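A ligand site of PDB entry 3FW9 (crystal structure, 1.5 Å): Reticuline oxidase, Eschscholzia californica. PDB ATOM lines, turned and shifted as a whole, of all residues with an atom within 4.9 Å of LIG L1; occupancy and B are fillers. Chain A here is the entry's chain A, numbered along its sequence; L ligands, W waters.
Water W3 bridges an oxygen (O2) of LIG L1 (2.6 Å) and an oxygen (O8) of LG2 L2 (3.0 Å). Water W1 lies within hydrogen-bond range of OD1 of Asn 365 (3.1 Å), O1 of LIG L1 (3.1 Å) and N of Met 157 (3.5 Å). Water W2 lies within hydrogen-bond range of N7 of LG2 L2, OE2 of Glu 392 and O2 of LIG L1.
NH2 of Arg 329 lies within salt-bridge range of OD2 of Asp 327, 2.6 Å away. The backbone NH (N) of Glu 392 sits at hydrogen-bond distance from the backbone carbonyl oxygen (O) of Ala 363 (2.9 Å). The side-chain amide oxygen (OD1) of Asn 365 lies within hydrogen-bond range of the side-chain hydroxyl (OG) of Ser 255 (2.6 Å). The backbone carbonyl oxygen of Ser 255 lies within hydrogen-bond range of the backbone NH of Leu 270. N of Phe 361 is in hydrogen-bond range of O of Ile 394.
The side-chain carboxylate (OD2) of Asp 327 sits at hydrogen-bond distance from an oxygen (O4) of LIG L1 (2.6 Å). A nitrogen (N1) of LIG L1 is in salt-bridge range of the side-chain carboxylate (OE1) of Glu 392 (3.5 Å). ND2 of Asn 365 is in hydrogen-bond range of O1 of LIG L1, 3.0 Å away. The backbone NH (N) of Trp 140 lies within hydrogen-bond range of an oxygen (O8) of LG2 L2 (2.9 Å). The side-chain sulfur (SG) of Cys 141 is bonded to a carbon (C15) of LG2 L2 (1.8 Å).
Merely in contact with LIG L1: Phe 331 (3.1 Å), Tyr 81 (3.1 Å), Leu 257 (3.2 Å), Trp 140 (3.5 Å), Met 157 (3.6 Å), Ser 255 (3.7 Å), Ala 363 (3.9 Å), Phe 361 (3.9 Å) and Cys 141 (3.9 Å).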
ATOM      1  N   TYR A  81      21.413  27.461 -31.972  1.00  0.00           N
ATOM      2  CA  TYR A  81      21.053  26.158 -31.448  1.00  0.00           C
ATOM      3  C   TYR A  81      19.852  25.568 -32.194  1.00  0.00           C
ATOM      4  O   TYR A  81      19.650  24.356 -32.204  1.00  0.00           O
ATOM      5  CB  TYR A  81      20.725  26.259 -29.960  1.00  0.00           C
ATOM      6  CG  TYR A  81      21.914  26.530 -29.066  1.00  0.00           C
ATOM      7  CD1 TYR A  81      23.222  26.309 -29.515  1.00  0.00           C
ATOM      8  CD2 TYR A  81      21.734  26.971 -27.765  1.00  0.00           C
ATOM      9  CE1 TYR A  81      24.310  26.552 -28.682  1.00  0.00           C
ATOM     10  CE2 TYR A  81      22.818  27.201 -26.930  1.00  0.00           C
ATOM     11  CZ  TYR A  81      24.102  26.998 -27.398  1.00  0.00           C
ATOM     12  OH  TYR A  81      25.172  27.224 -26.565  1.00  0.00           O
ATOM     13  N   TRP A 140      33.291  30.989 -24.944  1.00  0.00           N
ATOM     14  CA  TRP A 140      34.326  29.969 -24.797  1.00  0.00           C
ATOM     15  C   TRP A 140      34.569  29.231 -26.120  1.00  0.00           C
ATOM     16  O   TRP A 140      35.703  28.845 -26.425  1.00  0.00           O
ATOM     17  CB  TRP A 140      33.859  29.047 -23.666  1.00  0.00           C
ATOM     18  CG  TRP A 140      34.667  27.833 -23.323  1.00  0.00           C
ATOM     19  CD1 TRP A 140      35.703  27.764 -22.426  1.00  0.00           C
ATOM     20  CD2 TRP A 140      34.462  26.506 -23.806  1.00  0.00           C
ATOM     21  NE1 TRP A 140      36.162  26.471 -22.345  1.00  0.00           N
ATOM     22  CE2 TRP A 140      35.425  25.683 -23.179  1.00  0.00           C
ATOM     23  CE3 TRP A 140      33.566  25.932 -24.708  1.00  0.00           C
ATOM     24  CZ2 TRP A 140      35.513  24.312 -23.445  1.00  0.00           C
ATOM     25  CZ3 TRP A 140      33.649  24.579 -24.969  1.00  0.00           C
ATOM     26  CH2 TRP A 140      34.620  23.778 -24.335  1.00  0.00           C
ATOM     27  N   CYS A 141      33.519  29.046 -26.918  1.00  0.00           N
ATOM     28  CA  CYS A 141      33.638  28.323 -28.198  1.00  0.00           C
ATOM     29  C   CYS A 141      34.227  29.212 -29.296  1.00  0.00           C
ATOM     30  O   CYS A 141      33.632  30.226 -29.649  1.00  0.00           O
ATOM     31  CB  CYS A 141      32.261  27.802 -28.649  1.00  0.00           C
ATOM     32  SG  CYS A 141      31.363  26.689 -27.518  1.00  0.00           S
ATOM     33  N   MET A 157      34.504  33.180 -19.885  1.00  0.00           N
ATOM     34  CA  MET A 157      35.334  32.947 -18.707  1.00  0.00           C
ATOM     35  C   MET A 157      35.827  34.211 -18.028  1.00  0.00           C
ATOM     36  O   MET A 157      36.341  34.140 -16.912  1.00  0.00           O
ATOM     37  CB  MET A 157      36.534  32.073 -19.085  1.00  0.00           C
ATOM     38  CG  MET A 157      36.175  30.622 -19.389  1.00  0.00           C
ATOM     39  SD  MET A 157      35.603  29.669 -17.954  1.00  0.00           S
ATOM     40  CE  MET A 157      37.073  29.591 -16.934  1.00  0.00           C
ATOM     41  N   SER A 255      34.698  27.174 -13.458  1.00  0.00           N
ATOM     42  CA  SER A 255      33.551  26.584 -14.132  1.00  0.00           C
ATOM     43  C   SER A 255      33.716  25.083 -14.293  1.00  0.00           C
ATOM     44  O   SER A 255      34.806  24.548 -14.076  1.00  0.00           O
ATOM     45  CB  SER A 255      33.351  27.262 -15.486  1.00  0.00           C
ATOM     46  OG  SER A 255      33.044  28.636 -15.293  1.00  0.00           O
ATOM     47  N   LEU A 257      32.607  21.383 -16.584  1.00  0.00           N
ATOM     48  CA  LEU A 257      31.935  20.517 -17.543  1.00  0.00           C
ATOM     49  C   LEU A 257      31.801  19.147 -16.889  1.00  0.00           C
ATOM     50  O   LEU A 257      32.763  18.639 -16.324  1.00  0.00           O
ATOM     51  CB  LEU A 257      32.741  20.411 -18.828  1.00  0.00           C
ATOM     52  CG  LEU A 257      32.815  21.671 -19.687  1.00  0.00           C
ATOM     53  CD1 LEU A 257      33.879  21.523 -20.767  1.00  0.00           C
ATOM     54  CD2 LEU A 257      31.454  21.938 -20.314  1.00  0.00           C
ATOM     55  N   LEU A 270      37.447  23.986 -14.892  1.00  0.00           N
ATOM     56  CA  LEU A 270      38.069  25.013 -15.714  1.00  0.00           C
ATOM     57  C   LEU A 270      38.311  26.244 -14.870  1.00  0.00           C
ATOM     58  O   LEU A 270      37.373  26.919 -14.438  1.00  0.00           O
ATOM     59  CB  LEU A 270      37.146  25.383 -16.871  1.00  0.00           C
ATOM     60  CG  LEU A 270      36.757  24.221 -17.792  1.00  0.00           C
ATOM     61  CD1 LEU A 270      35.611  24.628 -18.719  1.00  0.00           C
ATOM     62  CD2 LEU A 270      37.948  23.755 -18.591  1.00  0.00           C
ATOM     63  N   PHE A 326      35.102  21.997 -34.285  1.00  0.00           N
ATOM     64  CA  PHE A 326      35.192  22.013 -32.836  1.00  0.00           C
ATOM     65  C   PHE A 326      34.469  20.812 -32.226  1.00  0.00           C
ATOM     66  O   PHE A 326      35.011  20.120 -31.357  1.00  0.00           O
ATOM     67  CB  PHE A 326      34.621  23.322 -32.268  1.00  0.00           C
ATOM     68  CG  PHE A 326      34.846  23.505 -30.797  1.00  0.00           C
ATOM     69  CD1 PHE A 326      33.777  23.473 -29.914  1.00  0.00           C
ATOM     70  CD2 PHE A 326      36.122  23.701 -30.282  1.00  0.00           C
ATOM     71  CE1 PHE A 326      33.973  23.640 -28.546  1.00  0.00           C
ATOM     72  CE2 PHE A 326      36.330  23.866 -28.936  1.00  0.00           C
ATOM     73  CZ  PHE A 326      35.255  23.833 -28.061  1.00  0.00           C
ATOM     74  N   ASP A 327      33.253  20.561 -32.698  1.00  0.00           N
ATOM     75  CA  ASP A 327      32.456  19.424 -32.234  1.00  0.00           C
ATOM     76  C   ASP A 327      31.418  19.105 -33.317  1.00  0.00           C
ATOM     77  O   ASP A 327      30.458  19.844 -33.495  1.00  0.00           O
ATOM     78  CB  ASP A 327      31.765  19.761 -30.910  1.00  0.00           C
ATOM     79  CG  ASP A 327      31.091  18.558 -30.274  1.00  0.00           C
ATOM     80  OD1 ASP A 327      30.840  17.572 -30.986  1.00  0.00           O
ATOM     81  OD2 ASP A 327      30.789  18.603 -29.056  1.00  0.00           O
ATOM     82  N   ARG A 329      29.012  17.038 -33.702  1.00  0.00           N
ATOM     83  CA  ARG A 329      27.834  16.282 -33.313  1.00  0.00           C
ATOM     84  C   ARG A 329      26.542  17.089 -33.404  1.00  0.00           C
ATOM     85  O   ARG A 329      26.525  18.278 -33.092  1.00  0.00           O
ATOM     86  CB  ARG A 329      27.996  15.727 -31.894  1.00  0.00           C
ATOM     87  CG  ARG A 329      29.029  14.629 -31.783  1.00  0.00           C
ATOM     88  CD  ARG A 329      29.967  14.873 -30.612  1.00  0.00           C
ATOM     89  NE  ARG A 329      29.369  14.551 -29.333  1.00  0.00           N
ATOM     90  CZ  ARG A 329      29.679  15.152 -28.189  1.00  0.00           C
ATOM     91  NH1 ARG A 329      29.094  14.794 -27.058  1.00  0.00           N
ATOM     92  NH2 ARG A 329      30.573  16.141 -28.176  1.00  0.00           N
ATOM     93  N   PHE A 331      23.140  18.176 -31.788  1.00  0.00           N
ATOM     94  CA  PHE A 331      22.856  18.352 -30.371  1.00  0.00           C
ATOM     95  C   PHE A 331      21.579  19.122 -30.109  1.00  0.00           C
ATOM     96  O   PHE A 331      21.072  19.844 -30.967  1.00  0.00           O
ATOM     97  CB  PHE A 331      24.031  19.040 -29.667  1.00  0.00           C
ATOM     98  CG  PHE A 331      24.239  20.476 -30.089  1.00  0.00           C
ATOM     99  CD1 PHE A 331      23.710  21.517 -29.339  1.00  0.00           C
ATOM    100  CD2 PHE A 331      24.978  20.764 -31.224  1.00  0.00           C
ATOM    101  CE1 PHE A 331      23.902  22.834 -29.736  1.00  0.00           C
ATOM    102  CE2 PHE A 331      25.186  22.075 -31.621  1.00  0.00           C
ATOM    103  CZ  PHE A 331      24.651  23.117 -30.879  1.00  0.00           C
ATOM    104  N   PHE A 361      25.787  15.910 -21.228  1.00  0.00           N
ATOM    105  CA  PHE A 361      26.742  16.586 -20.359  1.00  0.00           C
ATOM    106  C   PHE A 361      26.173  17.896 -19.842  1.00  0.00           C
ATOM    107  O   PHE A 361      25.153  18.380 -20.338  1.00  0.00           O
ATOM    108  CB  PHE A 361      28.133  16.743 -21.021  1.00  0.00           C
ATOM    109  CG  PHE A 361      28.181  17.686 -22.211  1.00  0.00           C
ATOM    110  CD1 PHE A 361      28.523  19.014 -22.045  1.00  0.00           C
ATOM    111  CD2 PHE A 361      27.941  17.217 -23.495  1.00  0.00           C
ATOM    112  CE1 PHE A 361      28.593  19.879 -23.151  1.00  0.00           C
ATOM    113  CE2 PHE A 361      28.009  18.061 -24.600  1.00  0.00           C
ATOM    114  CZ  PHE A 361      28.331  19.399 -24.419  1.00  0.00           C
ATOM    115  N   ALA A 363      27.190  21.998 -18.371  1.00  0.00           N
ATOM    116  CA  ALA A 363      28.182  23.064 -18.232  1.00  0.00           C
ATOM    117  C   ALA A 363      27.680  24.000 -17.140  1.00  0.00           C
ATOM    118  O   ALA A 363      26.543  24.458 -17.184  1.00  0.00           O
ATOM    119  CB  ALA A 363      28.371  23.812 -19.541  1.00  0.00           C
ATOM    120  N   ASN A 365      28.314  27.458 -14.690  1.00  0.00           N
ATOM    121  CA  ASN A 365      28.989  28.740 -14.524  1.00  0.00           C
ATOM    122  C   ASN A 365      28.379  29.537 -13.400  1.00  0.00           C
ATOM    123  O   ASN A 365      27.153  29.563 -13.239  1.00  0.00           O
ATOM    124  CB  ASN A 365      28.850  29.580 -15.799  1.00  0.00           C
ATOM    125  CG  ASN A 365      29.891  29.238 -16.822  1.00  0.00           C
ATOM    126  OD1 ASN A 365      31.063  29.600 -16.693  1.00  0.00           O
ATOM    127  ND2 ASN A 365      29.479  28.542 -17.877  1.00  0.00           N
ATOM    128  N   GLU A 392      23.756  24.618 -17.948  1.00  0.00           N
ATOM    129  CA  GLU A 392      23.422  24.157 -19.300  1.00  0.00           C
ATOM    130  C   GLU A 392      23.381  22.626 -19.342  1.00  0.00           C
ATOM    131  O   GLU A 392      24.245  21.959 -18.779  1.00  0.00           O
ATOM    132  CB  GLU A 392      24.451  24.692 -20.316  1.00  0.00           C
ATOM    133  CG  GLU A 392      24.581  26.212 -20.340  1.00  0.00           C
ATOM    134  CD  GLU A 392      25.743  26.675 -21.193  1.00  0.00           C
ATOM    135  OE1 GLU A 392      25.689  26.501 -22.431  1.00  0.00           O
ATOM    136  OE2 GLU A 392      26.711  27.222 -20.622  1.00  0.00           O
ATOM    137  N   ILE A 394      23.096  19.435 -22.082  1.00  0.00           N
ATOM    138  CA  ILE A 394      23.327  19.178 -23.497  1.00  0.00           C
ATOM    139  C   ILE A 394      23.276  17.682 -23.744  1.00  0.00           C
ATOM    140  O   ILE A 394      23.788  16.903 -22.953  1.00  0.00           O
ATOM    141  CB  ILE A 394      24.710  19.673 -23.965  1.00  0.00           C
ATOM    142  CG1 ILE A 394      24.915  21.157 -23.646  1.00  0.00           C
ATOM    143  CG2 ILE A 394      24.887  19.451 -25.464  1.00  0.00           C
ATOM    144  CD1 ILE A 394      25.451  21.423 -22.245  1.00  0.00           C
HETATM  145  C1  LIG L   1      29.294  23.473 -25.839  1.00  0.00           C
HETATM  146  C2  LIG L   1      30.273  22.578 -26.202  1.00  0.00           C
HETATM  147  C3  LIG L   1      30.018  21.594 -27.149  1.00  0.00           C
HETATM  148  C4  LIG L   1      28.788  21.495 -27.736  1.00  0.00           C
HETATM  149  C5  LIG L   1      27.754  22.388 -27.394  1.00  0.00           C
HETATM  150  C6  LIG L   1      28.011  23.400 -26.425  1.00  0.00           C
HETATM  151  C7  LIG L   1      26.859  24.223 -25.856  1.00  0.00           C
HETATM  152  C8  LIG L   1      27.412  25.497 -25.234  1.00  0.00           C
HETATM  153  N1  LIG L   1      28.362  25.041 -24.223  1.00  0.00           N
HETATM  154  C9  LIG L   1      29.589  24.491 -24.798  1.00  0.00           C
HETATM  155  C10 LIG L   1      30.415  23.796 -23.716  1.00  0.00           C
HETATM  156  C11 LIG L   1      30.731  24.823 -22.641  1.00  0.00           C
HETATM  157  C12 LIG L   1      31.883  24.698 -21.894  1.00  0.00           C
HETATM  158  C13 LIG L   1      32.176  25.636 -20.926  1.00  0.00           C
HETATM  159  C14 LIG L   1      31.276  26.719 -20.710  1.00  0.00           C
HETATM  160  O1  LIG L   1      31.540  27.626 -19.783  1.00  0.00           O
HETATM  161  C15 LIG L   1      32.830  27.634 -19.141  1.00  0.00           C
HETATM  162  C16 LIG L   1      30.155  26.829 -21.443  1.00  0.00           C
HETATM  163  O2  LIG L   1      29.299  27.883 -21.224  1.00  0.00           O
HETATM  164  C17 LIG L   1      29.869  25.914 -22.404  1.00  0.00           C
HETATM  165  C18 LIG L   1      28.601  26.070 -23.213  1.00  0.00           C
HETATM  166  O3  LIG L   1      28.595  20.512 -28.654  1.00  0.00           O
HETATM  167  C19 LIG L   1      27.654  20.660 -29.623  1.00  0.00           C
HETATM  168  O4  LIG L   1      31.000  20.727 -27.489  1.00  0.00           O
HETATM  169  P1  LG2 L   2      24.240  32.408 -36.255  1.00  0.00           P
HETATM  170  O1  LG2 L   2      23.459  31.121 -36.315  1.00  0.00           O
HETATM  171  O2  LG2 L   2      24.953  32.776 -37.533  1.00  0.00           O
HETATM  172  O3  LG2 L   2      23.315  33.641 -35.796  1.00  0.00           O
HETATM  173  C1  LG2 L   2      22.520  33.560 -34.619  1.00  0.00           C
HETATM  174  C2  LG2 L   2      21.341  34.517 -34.782  1.00  0.00           C
HETATM  175  O4  LG2 L   2      21.845  35.841 -34.976  1.00  0.00           O
HETATM  176  C3  LG2 L   2      20.474  34.230 -35.994  1.00  0.00           C
HETATM  177  O5  LG2 L   2      19.170  34.707 -35.711  1.00  0.00           O
HETATM  178  C4  LG2 L   2      21.087  35.100 -37.072  1.00  0.00           C
HETATM  179  O6  LG2 L   2      20.200  35.437 -38.132  1.00  0.00           O
HETATM  180  C5  LG2 L   2      21.502  36.318 -36.259  1.00  0.00           C
HETATM  181  N1  LG2 L   2      22.662  37.015 -36.835  1.00  0.00           N
HETATM  182  C6  LG2 L   2      23.852  36.467 -37.244  1.00  0.00           C
HETATM  183  N2  LG2 L   2      24.639  37.471 -37.702  1.00  0.00           N
HETATM  184  C7  LG2 L   2      23.982  38.640 -37.571  1.00  0.00           C
HETATM  185  C8  LG2 L   2      24.306  39.954 -37.867  1.00  0.00           C
HETATM  186  N3  LG2 L   2      25.506  40.271 -38.372  1.00  0.00           N
HETATM  187  N4  LG2 L   2      23.393  40.946 -37.604  1.00  0.00           N
HETATM  188  C9  LG2 L   2      22.166  40.642 -37.053  1.00  0.00           C
HETATM  189  N5  LG2 L   2      21.844  39.333 -36.771  1.00  0.00           N
HETATM  190  C10 LG2 L   2      22.735  38.365 -37.030  1.00  0.00           C
HETATM  191  N6  LG2 L   2      27.124  31.464 -26.014  1.00  0.00           N
HETATM  192  C11 LG2 L   2      27.668  32.157 -24.946  1.00  0.00           C
HETATM  193  O7  LG2 L   2      27.152  33.227 -24.570  1.00  0.00           O
HETATM  194  N7  LG2 L   2      28.842  31.715 -24.379  1.00  0.00           N
HETATM  195  C12 LG2 L   2      29.493  30.608 -24.869  1.00  0.00           C
HETATM  196  O8  LG2 L   2      30.529  30.230 -24.298  1.00  0.00           O
HETATM  197  C13 LG2 L   2      28.882  29.847 -25.873  1.00  0.00           C
HETATM  198  N8  LG2 L   2      29.500  28.713 -26.389  1.00  0.00           N
HETATM  199  C14 LG2 L   2      29.032  28.131 -27.551  1.00  0.00           C
HETATM  200  C15 LG2 L   2      29.728  27.083 -28.139  1.00  0.00           C
HETATM  201  C16 LG2 L   2      29.279  26.486 -29.303  1.00  0.00           C
HETATM  202  C17 LG2 L   2      30.023  25.309 -29.876  1.00  0.00           C
HETATM  203  C18 LG2 L   2      28.141  26.976 -29.935  1.00  0.00           C
HETATM  204  C19 LG2 L   2      27.668  26.396 -31.244  1.00  0.00           C
HETATM  205  C20 LG2 L   2      27.438  28.024 -29.355  1.00  0.00           C
HETATM  206  C21 LG2 L   2      27.880  28.600 -28.160  1.00  0.00           C
HETATM  207  N9  LG2 L   2      27.170  29.629 -27.550  1.00  0.00           N
HETATM  208  C22 LG2 L   2      27.718  30.299 -26.474  1.00  0.00           C
HETATM  209  C23 LG2 L   2      25.876  30.126 -28.152  1.00  0.00           C
HETATM  210  C24 LG2 L   2      26.121  31.317 -29.078  1.00  0.00           C
HETATM  211  O9  LG2 L   2      26.396  32.479 -28.309  1.00  0.00           O
HETATM  212  C25 LG2 L   2      24.884  31.581 -29.936  1.00  0.00           C
HETATM  213  O10 LG2 L   2      24.571  30.397 -30.663  1.00  0.00           O
HETATM  214  C26 LG2 L   2      25.156  32.742 -30.882  1.00  0.00           C
HETATM  215  O11 LG2 L   2      23.972  33.465 -31.154  1.00  0.00           O
HETATM  216  C27 LG2 L   2      25.763  32.232 -32.180  1.00  0.00           C
HETATM  217  O12 LG2 L   2      26.147  33.309 -33.034  1.00  0.00           O
HETATM  218  P2  LG2 L   2      26.586  32.944 -34.531  1.00  0.00           P
HETATM  219  O13 LG2 L   2      26.880  34.193 -35.319  1.00  0.00           O
HETATM  220  O14 LG2 L   2      27.648  31.894 -34.492  1.00  0.00           O
HETATM  221  O15 LG2 L   2      25.246  32.188 -35.034  1.00  0.00           O
HETATM  222  O   HOH W   1      32.192  30.663 -19.389  1.00  0.00           O
HETATM  223  O   HOH W   2      26.916  29.551 -22.997  1.00  0.00           O
HETATM  224  O   HOH W   3      30.183  30.338 -21.279  1.00  0.00           O
